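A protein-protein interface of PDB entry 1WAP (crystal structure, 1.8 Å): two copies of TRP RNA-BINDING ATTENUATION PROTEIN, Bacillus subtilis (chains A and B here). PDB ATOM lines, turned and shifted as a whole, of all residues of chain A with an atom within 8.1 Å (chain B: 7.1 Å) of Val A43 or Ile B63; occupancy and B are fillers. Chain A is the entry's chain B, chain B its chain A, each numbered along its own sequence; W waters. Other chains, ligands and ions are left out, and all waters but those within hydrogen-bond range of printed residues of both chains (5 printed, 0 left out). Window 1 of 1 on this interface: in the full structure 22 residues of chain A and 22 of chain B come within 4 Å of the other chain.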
ATOM      1  N   PHE A   9       3.866   3.992   3.316  1.00  0.00           N
ATOM      2  CA  PHE A   9       4.863   3.831   4.368  1.00  0.00           C
ATOM      3  C   PHE A   9       5.378   5.181   4.875  1.00  0.00           C
ATOM      4  O   PHE A   9       5.156   6.248   4.295  1.00  0.00           O
ATOM      5  CB  PHE A   9       6.016   2.928   3.877  1.00  0.00           C
ATOM      6  CG  PHE A   9       6.872   3.545   2.801  1.00  0.00           C
ATOM      7  CD1 PHE A   9       7.785   4.525   3.163  1.00  0.00           C
ATOM      8  CD2 PHE A   9       6.802   3.187   1.473  1.00  0.00           C
ATOM      9  CE1 PHE A   9       8.577   5.139   2.218  1.00  0.00           C
ATOM     10  CE2 PHE A   9       7.606   3.803   0.515  1.00  0.00           C
ATOM     11  CZ  PHE A   9       8.493   4.798   0.884  1.00  0.00           C
ATOM     12  N   VAL A  10       6.075   5.112   6.013  1.00  0.00           N
ATOM     13  CA  VAL A  10       6.689   6.269   6.649  1.00  0.00           C
ATOM     14  C   VAL A  10       8.172   5.981   6.873  1.00  0.00           C
ATOM     15  O   VAL A  10       8.571   4.832   7.150  1.00  0.00           O
ATOM     16  CB  VAL A  10       5.970   6.658   7.960  1.00  0.00           C
ATOM     17  CG1 VAL A  10       4.468   6.890   7.775  1.00  0.00           C
ATOM     18  CG2 VAL A  10       6.151   5.613   9.048  1.00  0.00           C
ATOM     19  N   VAL A  11       8.984   7.014   6.761  1.00  0.00           N
ATOM     20  CA  VAL A  11      10.428   6.927   7.012  1.00  0.00           C
ATOM     21  C   VAL A  11      10.716   7.632   8.326  1.00  0.00           C
ATOM     22  O   VAL A  11      10.299   8.790   8.463  1.00  0.00           O
ATOM     23  CB  VAL A  11      11.254   7.540   5.859  1.00  0.00           C
ATOM     24  CG1 VAL A  11      12.761   7.481   6.128  1.00  0.00           C
ATOM     25  CG2 VAL A  11      10.897   6.897   4.523  1.00  0.00           C
ATOM     26  N   ILE A  12      11.348   6.977   9.299  1.00  0.00           N
ATOM     27  CA  ILE A  12      11.627   7.614  10.594  1.00  0.00           C
ATOM     28  C   ILE A  12      13.126   7.495  10.925  1.00  0.00           C
ATOM     29  O   ILE A  12      13.633   6.364  10.882  1.00  0.00           O
ATOM     30  CB  ILE A  12      10.822   6.935  11.752  1.00  0.00           C
ATOM     31  CG1 ILE A  12       9.324   7.035  11.429  1.00  0.00           C
ATOM     32  CG2 ILE A  12      11.164   7.591  13.089  1.00  0.00           C
ATOM     33  CD1 ILE A  12       8.444   5.909  11.883  1.00  0.00           C
ATOM     34  N   LYS A  13      13.764   8.638  11.204  1.00  0.00           N
ATOM     35  CA  LYS A  13      15.178   8.570  11.609  1.00  0.00           C
ATOM     36  C   LYS A  13      15.305   9.054  13.061  1.00  0.00           C
ATOM     37  O   LYS A  13      14.822  10.171  13.313  1.00  0.00           O
ATOM     38  CB  LYS A  13      16.036   9.484  10.710  1.00  0.00           C
ATOM     39  CG  LYS A  13      17.507   9.505  11.128  1.00  0.00           C
ATOM     40  CD  LYS A  13      18.286  10.625  10.469  1.00  0.00           C
ATOM     41  CE  LYS A  13      19.711  10.594  11.009  1.00  0.00           C
ATOM     42  NZ  LYS A  13      20.484  11.647  10.259  1.00  0.00           N
ATOM     43  N   ALA A  14      15.876   8.252  13.954  1.00  0.00           N
ATOM     44  CA  ALA A  14      16.126   8.730  15.318  1.00  0.00           C
ATOM     45  C   ALA A  14      17.320   9.709  15.327  1.00  0.00           C
ATOM     46  O   ALA A  14      18.422   9.467  14.821  1.00  0.00           O
ATOM     47  CB  ALA A  14      16.386   7.572  16.255  1.00  0.00           C
ATOM     48  N   VAL A  21       9.068   3.683  17.957  1.00  0.00           N
ATOM     49  CA  VAL A  21       8.102   3.575  16.860  1.00  0.00           C
ATOM     50  C   VAL A  21       7.106   2.476  17.209  1.00  0.00           C
ATOM     51  O   VAL A  21       7.393   1.271  17.238  1.00  0.00           O
ATOM     52  CB  VAL A  21       8.851   3.352  15.526  1.00  0.00           C
ATOM     53  CG1 VAL A  21       7.863   3.300  14.363  1.00  0.00           C
ATOM     54  CG2 VAL A  21       9.885   4.454  15.304  1.00  0.00           C
ATOM     55  N   GLU A  36       8.999  -0.479  18.563  1.00  0.00           N
ATOM     56  CA  GLU A  36      10.352  -0.678  18.023  1.00  0.00           C
ATOM     57  C   GLU A  36      11.248   0.424  18.564  1.00  0.00           C
ATOM     58  O   GLU A  36      10.941   1.591  18.375  1.00  0.00           O
ATOM     59  CB  GLU A  36      10.414  -0.711  16.509  1.00  0.00           C
ATOM     60  CG  GLU A  36      11.775  -1.109  15.952  1.00  0.00           C
ATOM     61  CD  GLU A  36      12.181  -2.550  16.192  1.00  0.00           C
ATOM     62  OE1 GLU A  36      11.412  -3.508  16.286  1.00  0.00           O
ATOM     63  OE2 GLU A  36      13.417  -2.726  16.252  1.00  0.00           O
ATOM     64  N   LEU A  38      14.466   2.661  18.491  1.00  0.00           N
ATOM     65  CA  LEU A  38      15.439   3.121  17.489  1.00  0.00           C
ATOM     66  C   LEU A  38      16.525   3.932  18.198  1.00  0.00           C
ATOM     67  O   LEU A  38      16.164   4.964  18.782  1.00  0.00           O
ATOM     68  CB  LEU A  38      14.730   4.056  16.519  1.00  0.00           C
ATOM     69  CG  LEU A  38      14.203   3.679  15.174  1.00  0.00           C
ATOM     70  CD1 LEU A  38      14.077   4.966  14.313  1.00  0.00           C
ATOM     71  CD2 LEU A  38      15.060   2.695  14.420  1.00  0.00           C
ATOM     72  N   ASP A  39      17.776   3.511  18.143  1.00  0.00           N
ATOM     73  CA  ASP A  39      18.842   4.352  18.696  1.00  0.00           C
ATOM     74  C   ASP A  39      19.264   5.438  17.701  1.00  0.00           C
ATOM     75  O   ASP A  39      18.904   5.485  16.523  1.00  0.00           O
ATOM     76  CB  ASP A  39      19.959   3.469  19.207  1.00  0.00           C
ATOM     77  CG  ASP A  39      19.532   2.615  20.401  1.00  0.00           C
ATOM     78  OD1 ASP A  39      18.702   3.080  21.216  1.00  0.00           O
ATOM     79  OD2 ASP A  39      20.045   1.481  20.498  1.00  0.00           O
ATOM     80  N   LYS A  40      20.046   6.375  18.205  1.00  0.00           N
ATOM     81  CA  LYS A  40      20.467   7.570  17.485  1.00  0.00           C
ATOM     82  C   LYS A  40      21.100   7.264  16.138  1.00  0.00           C
ATOM     83  O   LYS A  40      22.046   6.455  16.106  1.00  0.00           O
ATOM     84  CB  LYS A  40      21.502   8.246  18.390  1.00  0.00           C
ATOM     85  CG  LYS A  40      21.814   9.625  17.858  1.00  0.00           C
ATOM     86  CD  LYS A  40      22.897  10.255  18.756  1.00  0.00           C
ATOM     87  CE  LYS A  40      22.983  11.732  18.417  1.00  0.00           C
ATOM     88  NZ  LYS A  40      23.856  12.428  19.414  1.00  0.00           N
ATOM     89  N   GLY A  41      20.572   7.842  15.058  1.00  0.00           N
ATOM     90  CA  GLY A  41      21.129   7.602  13.734  1.00  0.00           C
ATOM     91  C   GLY A  41      20.492   6.460  12.950  1.00  0.00           C
ATOM     92  O   GLY A  41      20.805   6.335  11.748  1.00  0.00           O
ATOM     93  N   GLU A  42      19.657   5.624  13.557  1.00  0.00           N
ATOM     94  CA  GLU A  42      19.075   4.493  12.823  1.00  0.00           C
ATOM     95  C   GLU A  42      17.792   4.974  12.133  1.00  0.00           C
ATOM     96  O   GLU A  42      17.185   5.939  12.595  1.00  0.00           O
ATOM     97  CB  GLU A  42      18.683   3.346  13.767  1.00  0.00           C
ATOM     98  CG  GLU A  42      19.896   2.709  14.412  1.00  0.00           C
ATOM     99  CD  GLU A  42      19.564   1.694  15.480  1.00  0.00           C
ATOM    100  OE1 GLU A  42      18.431   1.560  15.960  1.00  0.00           O
ATOM    101  OE2 GLU A  42      20.616   1.083  15.797  1.00  0.00           O
ATOM    102  N   VAL A  43      17.422   4.279  11.083  1.00  0.00           N
ATOM    103  CA  VAL A  43      16.262   4.626  10.277  1.00  0.00           C
ATOM    104  C   VAL A  43      15.351   3.389  10.157  1.00  0.00           C
ATOM    105  O   VAL A  43      15.844   2.246  10.000  1.00  0.00           O
ATOM    106  CB  VAL A  43      16.726   5.100   8.862  1.00  0.00           C
ATOM    107  CG1 VAL A  43      15.490   5.339   7.991  1.00  0.00           C
ATOM    108  CG2 VAL A  43      17.592   6.362   8.955  1.00  0.00           C
ATOM    109  N   ILE A  44      14.048   3.627  10.300  1.00  0.00           N
ATOM    110  CA  ILE A  44      13.078   2.580   9.918  1.00  0.00           C
ATOM    111  C   ILE A  44      12.125   3.084   8.842  1.00  0.00           C
ATOM    112  O   ILE A  44      11.666   4.217   8.899  1.00  0.00           O
ATOM    113  CB  ILE A  44      12.363   1.988  11.149  1.00  0.00           C
ATOM    114  CG1 ILE A  44      11.504   0.776  10.710  1.00  0.00           C
ATOM    115  CG2 ILE A  44      11.516   3.014  11.892  1.00  0.00           C
ATOM    116  CD1 ILE A  44      11.114  -0.102  11.917  1.00  0.00           C
ATOM    117  N   ILE A  45      11.857   2.253   7.859  1.00  0.00           N
ATOM    118  CA  ILE A  45      10.842   2.503   6.852  1.00  0.00           C
ATOM    119  C   ILE A  45       9.701   1.506   7.136  1.00  0.00           C
ATOM    120  O   ILE A  45       9.917   0.285   6.983  1.00  0.00           O
ATOM    121  CB  ILE A  45      11.389   2.326   5.422  1.00  0.00           C
ATOM    122  CG1 ILE A  45      12.715   3.091   5.205  1.00  0.00           C
ATOM    123  CG2 ILE A  45      10.359   2.809   4.379  1.00  0.00           C
ATOM    124  CD1 ILE A  45      13.997   2.285   5.404  1.00  0.00           C
ATOM    125  N   ALA A  46       8.526   2.006   7.529  1.00  0.00           N
ATOM    126  CA  ALA A  46       7.462   1.081   7.979  1.00  0.00           C
ATOM    127  C   ALA A  46       6.157   1.290   7.229  1.00  0.00           C
ATOM    128  O   ALA A  46       5.731   2.437   7.069  1.00  0.00           O
ATOM    129  CB  ALA A  46       7.249   1.284   9.472  1.00  0.00           C
ATOM    130  N   LEU A  62      13.142  12.495  12.899  1.00  0.00           N
ATOM    131  CA  LEU A  62      12.721  13.130  11.659  1.00  0.00           C
ATOM    132  C   LEU A  62      11.838  12.124  10.913  1.00  0.00           C
ATOM    133  O   LEU A  62      12.199  10.943  10.825  1.00  0.00           O
ATOM    134  CB  LEU A  62      13.971  13.509  10.844  1.00  0.00           C
ATOM    135  CG  LEU A  62      13.713  14.218   9.517  1.00  0.00           C
ATOM    136  CD1 LEU A  62      13.174  15.636   9.724  1.00  0.00           C
ATOM    137  CD2 LEU A  62      14.956  14.216   8.641  1.00  0.00           C
ATOM    138  N   GLN A  64       9.514  11.412   7.319  1.00  0.00           N
ATOM    139  CA  GLN A  64       9.116  11.708   5.952  1.00  0.00           C
ATOM    140  C   GLN A  64       7.943  10.811   5.522  1.00  0.00           C
ATOM    141  O   GLN A  64       7.930   9.593   5.726  1.00  0.00           O
ATOM    142  CB  GLN A  64      10.202  11.510   4.896  1.00  0.00           C
ATOM    143  CG  GLN A  64      11.463  12.317   5.055  1.00  0.00           C
ATOM    144  CD  GLN A  64      12.570  11.843   4.129  1.00  0.00           C
ATOM    145  OE1 GLN A  64      12.606  10.664   3.763  1.00  0.00           O
ATOM    146  NE2 GLN A  64      13.472  12.749   3.802  1.00  0.00           N
ATOM    147  N   VAL B  10      13.018   0.575  -1.506  1.00  0.00           N
ATOM    148  CA  VAL B  10      13.919   1.554  -0.934  1.00  0.00           C
ATOM    149  C   VAL B  10      15.314   1.251  -1.478  1.00  0.00           C
ATOM    150  O   VAL B  10      15.649   0.082  -1.702  1.00  0.00           O
ATOM    151  CB  VAL B  10      13.858   1.617   0.600  1.00  0.00           C
ATOM    152  CG1 VAL B  10      12.439   1.567   1.156  1.00  0.00           C
ATOM    153  CG2 VAL B  10      14.670   0.521   1.231  1.00  0.00           C
ATOM    154  N   VAL B  11      16.085   2.311  -1.708  1.00  0.00           N
ATOM    155  CA  VAL B  11      17.466   2.166  -2.191  1.00  0.00           C
ATOM    156  C   VAL B  11      18.381   2.607  -1.044  1.00  0.00           C
ATOM    157  O   VAL B  11      18.146   3.637  -0.431  1.00  0.00           O
ATOM    158  CB  VAL B  11      17.699   3.065  -3.420  1.00  0.00           C
ATOM    159  CG1 VAL B  11      19.118   2.892  -3.942  1.00  0.00           C
ATOM    160  CG2 VAL B  11      16.671   2.717  -4.492  1.00  0.00           C
ATOM    161  N   ILE B  12      19.302   1.709  -0.718  1.00  0.00           N
ATOM    162  CA  ILE B  12      20.273   1.932   0.358  1.00  0.00           C
ATOM    163  C   ILE B  12      21.684   1.715  -0.135  1.00  0.00           C
ATOM    164  O   ILE B  12      22.059   0.670  -0.674  1.00  0.00           O
ATOM    165  CB  ILE B  12      20.012   0.994   1.602  1.00  0.00           C
ATOM    166  CG1 ILE B  12      18.591   1.304   2.128  1.00  0.00           C
ATOM    167  CG2 ILE B  12      21.062   1.275   2.703  1.00  0.00           C
ATOM    168  CD1 ILE B  12      17.834   0.076   2.547  1.00  0.00           C
ATOM    169  N   LYS B  13      22.528   2.735   0.069  1.00  0.00           N
ATOM    170  CA  LYS B  13      23.947   2.617  -0.206  1.00  0.00           C
ATOM    171  C   LYS B  13      24.798   2.682   1.081  1.00  0.00           C
ATOM    172  O   LYS B  13      24.665   3.627   1.860  1.00  0.00           O
ATOM    173  CB  LYS B  13      24.399   3.818  -1.088  1.00  0.00           C
ATOM    174  CG  LYS B  13      25.919   3.730  -1.340  1.00  0.00           C
ATOM    175  CD  LYS B  13      26.477   4.967  -2.012  1.00  0.00           C
ATOM    176  CE  LYS B  13      27.979   4.823  -2.276  1.00  0.00           C
ATOM    177  NZ  LYS B  13      28.358   5.905  -3.244  1.00  0.00           N
ATOM    178  N   ILE B  55      11.450  -2.105   7.282  1.00  0.00           N
ATOM    179  CA  ILE B  55      12.870  -2.279   7.001  1.00  0.00           C
ATOM    180  C   ILE B  55      13.630  -1.323   7.930  1.00  0.00           C
ATOM    181  O   ILE B  55      13.280  -0.129   7.998  1.00  0.00           O
ATOM    182  CB  ILE B  55      13.202  -2.010   5.511  1.00  0.00           C
ATOM    183  CG1 ILE B  55      12.518  -3.042   4.611  1.00  0.00           C
ATOM    184  CG2 ILE B  55      14.725  -1.969   5.279  1.00  0.00           C
ATOM    185  CD1 ILE B  55      12.532  -2.724   3.106  1.00  0.00           C
ATOM    186  N   LYS B  56      14.633  -1.901   8.624  1.00  0.00           N
ATOM    187  CA  LYS B  56      15.445  -1.072   9.534  1.00  0.00           C
ATOM    188  C   LYS B  56      16.864  -0.971   8.971  1.00  0.00           C
ATOM    189  O   LYS B  56      17.385  -1.955   8.442  1.00  0.00           O
ATOM    190  CB  LYS B  56      15.392  -1.607  10.935  1.00  0.00           C
ATOM    191  CG  LYS B  56      16.026  -0.846  12.067  1.00  0.00           C
ATOM    192  CD  LYS B  56      15.803  -1.689  13.368  1.00  0.00           C
ATOM    193  CE  LYS B  56      16.092  -0.783  14.549  1.00  0.00           C
ATOM    194  NZ  LYS B  56      16.000  -1.429  15.874  1.00  0.00           N
ATOM    195  N   VAL B  57      17.456   0.218   9.028  1.00  0.00           N
ATOM    196  CA  VAL B  57      18.828   0.449   8.559  1.00  0.00           C
ATOM    197  C   VAL B  57      19.693   0.880   9.740  1.00  0.00           C
ATOM    198  O   VAL B  57      19.323   1.819  10.438  1.00  0.00           O
ATOM    199  CB  VAL B  57      18.891   1.456   7.396  1.00  0.00           C
ATOM    200  CG1 VAL B  57      20.320   1.588   6.860  1.00  0.00           C
ATOM    201  CG2 VAL B  57      17.915   1.015   6.298  1.00  0.00           C
ATOM    202  N   ARG B  58      20.815   0.183   9.910  1.00  0.00           N
ATOM    203  CA  ARG B  58      21.765   0.466  10.988  1.00  0.00           C
ATOM    204  C   ARG B  58      23.171   0.631  10.417  1.00  0.00           C
ATOM    205  O   ARG B  58      23.639  -0.226   9.652  1.00  0.00           O
ATOM    206  CB  ARG B  58      21.645  -0.668  11.981  1.00  0.00           C
ATOM    207  CG  ARG B  58      22.456  -0.660  13.255  1.00  0.00           C
ATOM    208  CD  ARG B  58      22.150  -1.944  14.060  1.00  0.00           C
ATOM    209  NE  ARG B  58      20.858  -1.873  14.718  1.00  0.00           N
ATOM    210  CZ  ARG B  58      20.002  -2.777  15.172  1.00  0.00           C
ATOM    211  NH1 ARG B  58      20.197  -4.097  15.064  1.00  0.00           N
ATOM    212  NH2 ARG B  58      18.855  -2.401  15.773  1.00  0.00           N
ATOM    213  N   GLY B  59      23.849   1.728  10.736  1.00  0.00           N
ATOM    214  CA  GLY B  59      25.195   2.024  10.226  1.00  0.00           C
ATOM    215  C   GLY B  59      25.178   3.261   9.337  1.00  0.00           C
ATOM    216  O   GLY B  59      24.116   3.862   9.142  1.00  0.00           O
ATOM    217  N   ALA B  61      24.826   5.193   6.082  1.00  0.00           N
ATOM    218  CA  ALA B  61      24.263   4.858   4.779  1.00  0.00           C
ATOM    219  C   ALA B  61      23.428   6.002   4.223  1.00  0.00           C
ATOM    220  O   ALA B  61      23.008   6.835   4.995  1.00  0.00           O
ATOM    221  CB  ALA B  61      23.331   3.634   4.873  1.00  0.00           C
ATOM    222  N   LEU B  62      23.233   5.981   2.918  1.00  0.00           N
ATOM    223  CA  LEU B  62      22.296   6.918   2.290  1.00  0.00           C
ATOM    224  C   LEU B  62      21.092   6.115   1.790  1.00  0.00           C
ATOM    225  O   LEU B  62      21.268   5.059   1.175  1.00  0.00           O
ATOM    226  CB  LEU B  62      22.982   7.671   1.153  1.00  0.00           C
ATOM    227  CG  LEU B  62      22.104   8.658   0.391  1.00  0.00           C
ATOM    228  CD1 LEU B  62      21.610   9.842   1.197  1.00  0.00           C
ATOM    229  CD2 LEU B  62      22.874   9.096  -0.842  1.00  0.00           C
ATOM    230  N   ILE B  63      19.916   6.597   2.134  1.00  0.00           N
ATOM    231  CA  ILE B  63      18.638   5.975   1.833  1.00  0.00           C
ATOM    232  C   ILE B  63      17.861   6.879   0.883  1.00  0.00           C
ATOM    233  O   ILE B  63      17.800   8.093   1.127  1.00  0.00           O
ATOM    234  CB  ILE B  63      17.828   5.739   3.137  1.00  0.00           C
ATOM    235  CG1 ILE B  63      18.639   4.812   4.063  1.00  0.00           C
ATOM    236  CG2 ILE B  63      16.424   5.164   2.913  1.00  0.00           C
ATOM    237  CD1 ILE B  63      18.304   4.890   5.518  1.00  0.00           C
ATOM    238  N   GLN B  64      17.315   6.257  -0.163  1.00  0.00           N
ATOM    239  CA  GLN B  64      16.423   6.994  -1.068  1.00  0.00           C
ATOM    240  C   GLN B  64      15.083   6.254  -1.134  1.00  0.00           C
ATOM    241  O   GLN B  64      15.060   5.043  -1.358  1.00  0.00           O
ATOM    242  CB  GLN B  64      16.877   7.044  -2.537  1.00  0.00           C
ATOM    243  CG  GLN B  64      18.141   7.817  -2.799  1.00  0.00           C
ATOM    244  CD  GLN B  64      18.594   7.604  -4.237  1.00  0.00           C
ATOM    245  OE1 GLN B  64      18.311   6.581  -4.855  1.00  0.00           O
ATOM    246  NE2 GLN B  64      19.316   8.588  -4.734  1.00  0.00           N
ATOM    247  N   THR B  65      14.007   7.015  -1.013  1.00  0.00           N
ATOM    248  CA  THR B  65      12.677   6.441  -1.211  1.00  0.00           C
ATOM    249  C   THR B  65      11.860   7.435  -2.066  1.00  0.00           C
ATOM    250  O   THR B  65      12.342   8.469  -2.498  1.00  0.00           O
ATOM    251  CB  THR B  65      11.898   6.252   0.126  1.00  0.00           C
ATOM    252  OG1 THR B  65      11.575   7.580   0.589  1.00  0.00           O
ATOM    253  CG2 THR B  65      12.706   5.466   1.139  1.00  0.00           C
ATOM    254  N   GLY B  68      12.209  11.143  -0.876  1.00  0.00           N
ATOM    255  CA  GLY B  68      13.512  11.777  -0.793  1.00  0.00           C
ATOM    256  C   GLY B  68      14.633  10.899  -0.223  1.00  0.00           C
ATOM    257  O   GLY B  68      14.602   9.671  -0.244  1.00  0.00           O
ATOM    258  N   GLU B  69      15.638  11.588   0.310  1.00  0.00           N
ATOM    259  CA  GLU B  69      16.814  11.033   0.931  1.00  0.00           C
ATOM    260  C   GLU B  69      16.888  11.212   2.447  1.00  0.00           C
ATOM    261  O   GLU B  69      16.512  12.242   3.029  1.00  0.00           O
ATOM    262  CB  GLU B  69      18.079  11.653   0.346  1.00  0.00           C
ATOM    263  CG  GLU B  69      18.136  11.581  -1.167  1.00  0.00           C
ATOM    264  CD  GLU B  69      19.518  11.752  -1.761  1.00  0.00           C
ATOM    265  OE1 GLU B  69      20.293  12.573  -1.234  1.00  0.00           O
ATOM    266  OE2 GLU B  69      19.802  11.041  -2.762  1.00  0.00           O
ATOM    267  N   MET B  70      17.418  10.179   3.088  1.00  0.00           N
ATOM    268  CA  MET B  70      17.607  10.120   4.551  1.00  0.00           C
ATOM    269  C   MET B  70      18.983   9.483   4.788  1.00  0.00           C
ATOM    270  O   MET B  70      19.320   8.506   4.089  1.00  0.00           O
ATOM    271  CB  MET B  70      16.458   9.298   5.171  1.00  0.00           C
ATOM    272  CG  MET B  70      16.400   9.257   6.684  1.00  0.00           C
ATOM    273  SD  MET B  70      15.920  10.892   7.326  1.00  0.00           S
ATOM    274  CE  MET B  70      14.131  10.687   7.285  1.00  0.00           C
ATOM    275  N   LYS B  71      19.820   9.997   5.676  1.00  0.00           N
ATOM    276  CA  LYS B  71      21.077   9.353   6.003  1.00  0.00           C
ATOM    277  C   LYS B  71      20.949   8.619   7.337  1.00  0.00           C
ATOM    278  O   LYS B  71      20.412   9.240   8.258  1.00  0.00           O
ATOM    279  CB  LYS B  71      22.174  10.405   6.158  1.00  0.00           C
ATOM    280  CG  LYS B  71      22.253  11.310   4.933  1.00  0.00           C
ATOM    281  CD  LYS B  71      23.603  12.020   4.913  1.00  0.00           C
ATOM    282  CE  LYS B  71      23.631  13.268   4.042  1.00  0.00           C
ATOM    283  NZ  LYS B  71      24.947  13.978   4.181  1.00  0.00           N
ATOM    284  N   SER B  72      21.360   7.357   7.409  1.00  0.00           N
ATOM    285  CA  SER B  72      21.512   6.717   8.714  1.00  0.00           C
ATOM    286  C   SER B  72      22.956   7.035   9.129  1.00  0.00           C
ATOM    287  O   SER B  72      23.796   7.231   8.252  1.00  0.00           O
ATOM    288  CB  SER B  72      21.256   5.214   8.682  1.00  0.00           C
ATOM    289  OG  SER B  72      22.011   4.616   7.660  1.00  0.00           O
ATOM    290  N   GLU B  73      23.188   7.092  10.419  1.00  0.00           N
ATOM    291  CA  GLU B  73      24.569   7.290  10.897  1.00  0.00           C
ATOM    292  C   GLU B  73      25.020   6.211  11.847  1.00  0.00           C
ATOM    293  O   GLU B  73      24.207   5.827  12.706  1.00  0.00           O
ATOM    294  CB  GLU B  73      24.575   8.642  11.655  1.00  0.00           C
ATOM    295  CG  GLU B  73      23.701   9.597  10.854  1.00  0.00           C
ATOM    296  CD  GLU B  73      23.817  11.005  11.355  1.00  0.00           C
ATOM    297  OE1 GLU B  73      24.960  11.390  11.680  1.00  0.00           O
ATOM    298  OE2 GLU B  73      22.748  11.646  11.368  1.00  0.00           O
HETATM  299  O   HOH W   1      13.445   8.594   2.333  1.00  0.00           O
HETATM  300  O   HOH W   2      17.740  -0.328  17.537  1.00  0.00           O
HETATM  301  O   HOH W   3      21.197  11.324  13.980  1.00  0.00           O
HETATM  302  O   HOH W   4      22.658   3.657  12.483  1.00  0.00           O
HETATM  303  O   HOH W   5      24.800   7.602  15.409  1.00  0.00           O
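The backbone carbonyl oxygen of Ile B55 lies within hydrogen-bond range of the backbone NH of Ile A45 (2.8 Å). The side-chain amino group (NZ) of Lys B56 is in salt-bridge range of the side-chain carboxylate (OE2) of Glu A36 (2.9 Å). The side-chain carboxylate (OE1) of Glu A42 is in salt-bridge range of the side-chain amino group (NZ) of Lys B56. N of Val B57 is in hydrogen-bond range of O of Val A43 (2.8 Å). The guanidinium group of Arg B58 lies within salt-bridge range of the side-chain carboxylate of Glu A42 (3.2 Å). The backbone carbonyl oxygen (O) of Glu B69 lies within hydrogen-bond range of the side-chain amide nitrogen (NE2) of Gln A64, 3.2 Å away. The backbone carbonyl oxygen (O) of Lys B71 sits at hydrogen-bond distance from the side-chain amino group (NZ) of Lys A13 (3.1 Å). OE2 of Glu B73 lies within salt-bridge range of NZ of Lys A13 (2.5 Å). N of Glu B73 lies within hydrogen-bond range of O of Gly A41, at 2.8 Å.
CZ of Phe A9 touches CB of Thr B65 (3.8 Å). Met B70 touches Val A11. CD2 of Leu A38 touches CE of Lys B56 (3.6 Å). Gly A41 touches Ser B72 (O to CA, 3.1 Å). CA of Glu A42 touches O of Val B57, at 3.6 Å. CD2 of Leu A62 touches SD of Met B70, at 3.7 Å. Gln A64 touches Met B70.
The backbone carbonyl oxygen (O) of Met B70 lies within hydrogen-bond range of the backbone NH (N) of Ile B63 (2.8 Å). O of Val A21 sits at hydrogen-bond distance from N of Glu A36 (2.7 Å). The backbone NH (N) of Asp A39 sits at hydrogen-bond distance from the side-chain carboxylate (OE1) of Glu A42 (3.0 Å).
Water W2 lies within hydrogen-bond range of the side-chain carboxylate of Glu A42, the side-chain amino group of Lys B56 and the guanidinium group of Arg B58. Water W3 lies within hydrogen-bond range of the side-chain carboxylate of Glu B73 (3.1 Å) and the backbone carbonyl oxygen of Ala A14 (3.4 Å).
Positions printed for both chains: 10, 11, 12, 13, 62 and 64. Of the 22 pairs that touch across the chains among the printed residues, none has its exchanged pair printed and touching as well.
Hydrophobic or aromatic side chains of chain A within 4 Å of the printed part of chain B: Phe A9, Val A11, Leu A38, Val A43, Ile A44, Ile A45 and Leu A62. Of the 20 printed residues of chain B, 11 touch a printed residue of chain A. Printed residues of chain B that touch a printed residue of chain A: Ile B55, Lys B56, Val B57, Arg B58, Ile B63, Thr B65, Glu B69, Met B70, Lys B71, Ser B72 and Glu B73. Hydrophobic or aromatic side chains of chain B that line the printed part of chain A: Ile B63 and Met B70. Along chain B the printed residues that touch a printed residue of chain A span positions 55 to 73. Among the printed residues, 22 pairs touch across the chains. Among the printed residues, Asp or Glu carboxylates within 4 Å of a Lys or Arg side-chain nitrogen of the other chain: Lys A13 with Glu B73, Glu A36 with Lys B56, Glu A42 with Lys B56 and Glu A42 with Arg B58.
Val A10 touches none of the printed residues of chain B. Lys A40 touches none of the printed residues of chain B. Printed residues of chain B within 4 Å of Glu A42: Lys B56, Val B57 and Arg B58. Val A43 touches just these residues of chain B: Lys B56 (3.4 Å), Val B57 (2.8 Å), Ile B63 (3.7 Å), Met B70 (3.9 Å) and Ser B72 (3.8 Å). Of the printed residues of chain A, Ile B55 touches Ile A44 and Ile A45. Ile B63 touches just one residue of chain A: Val A43. The nearest residue of chain B that does not touch Val A43 is Ile B55 (4.03 Å).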
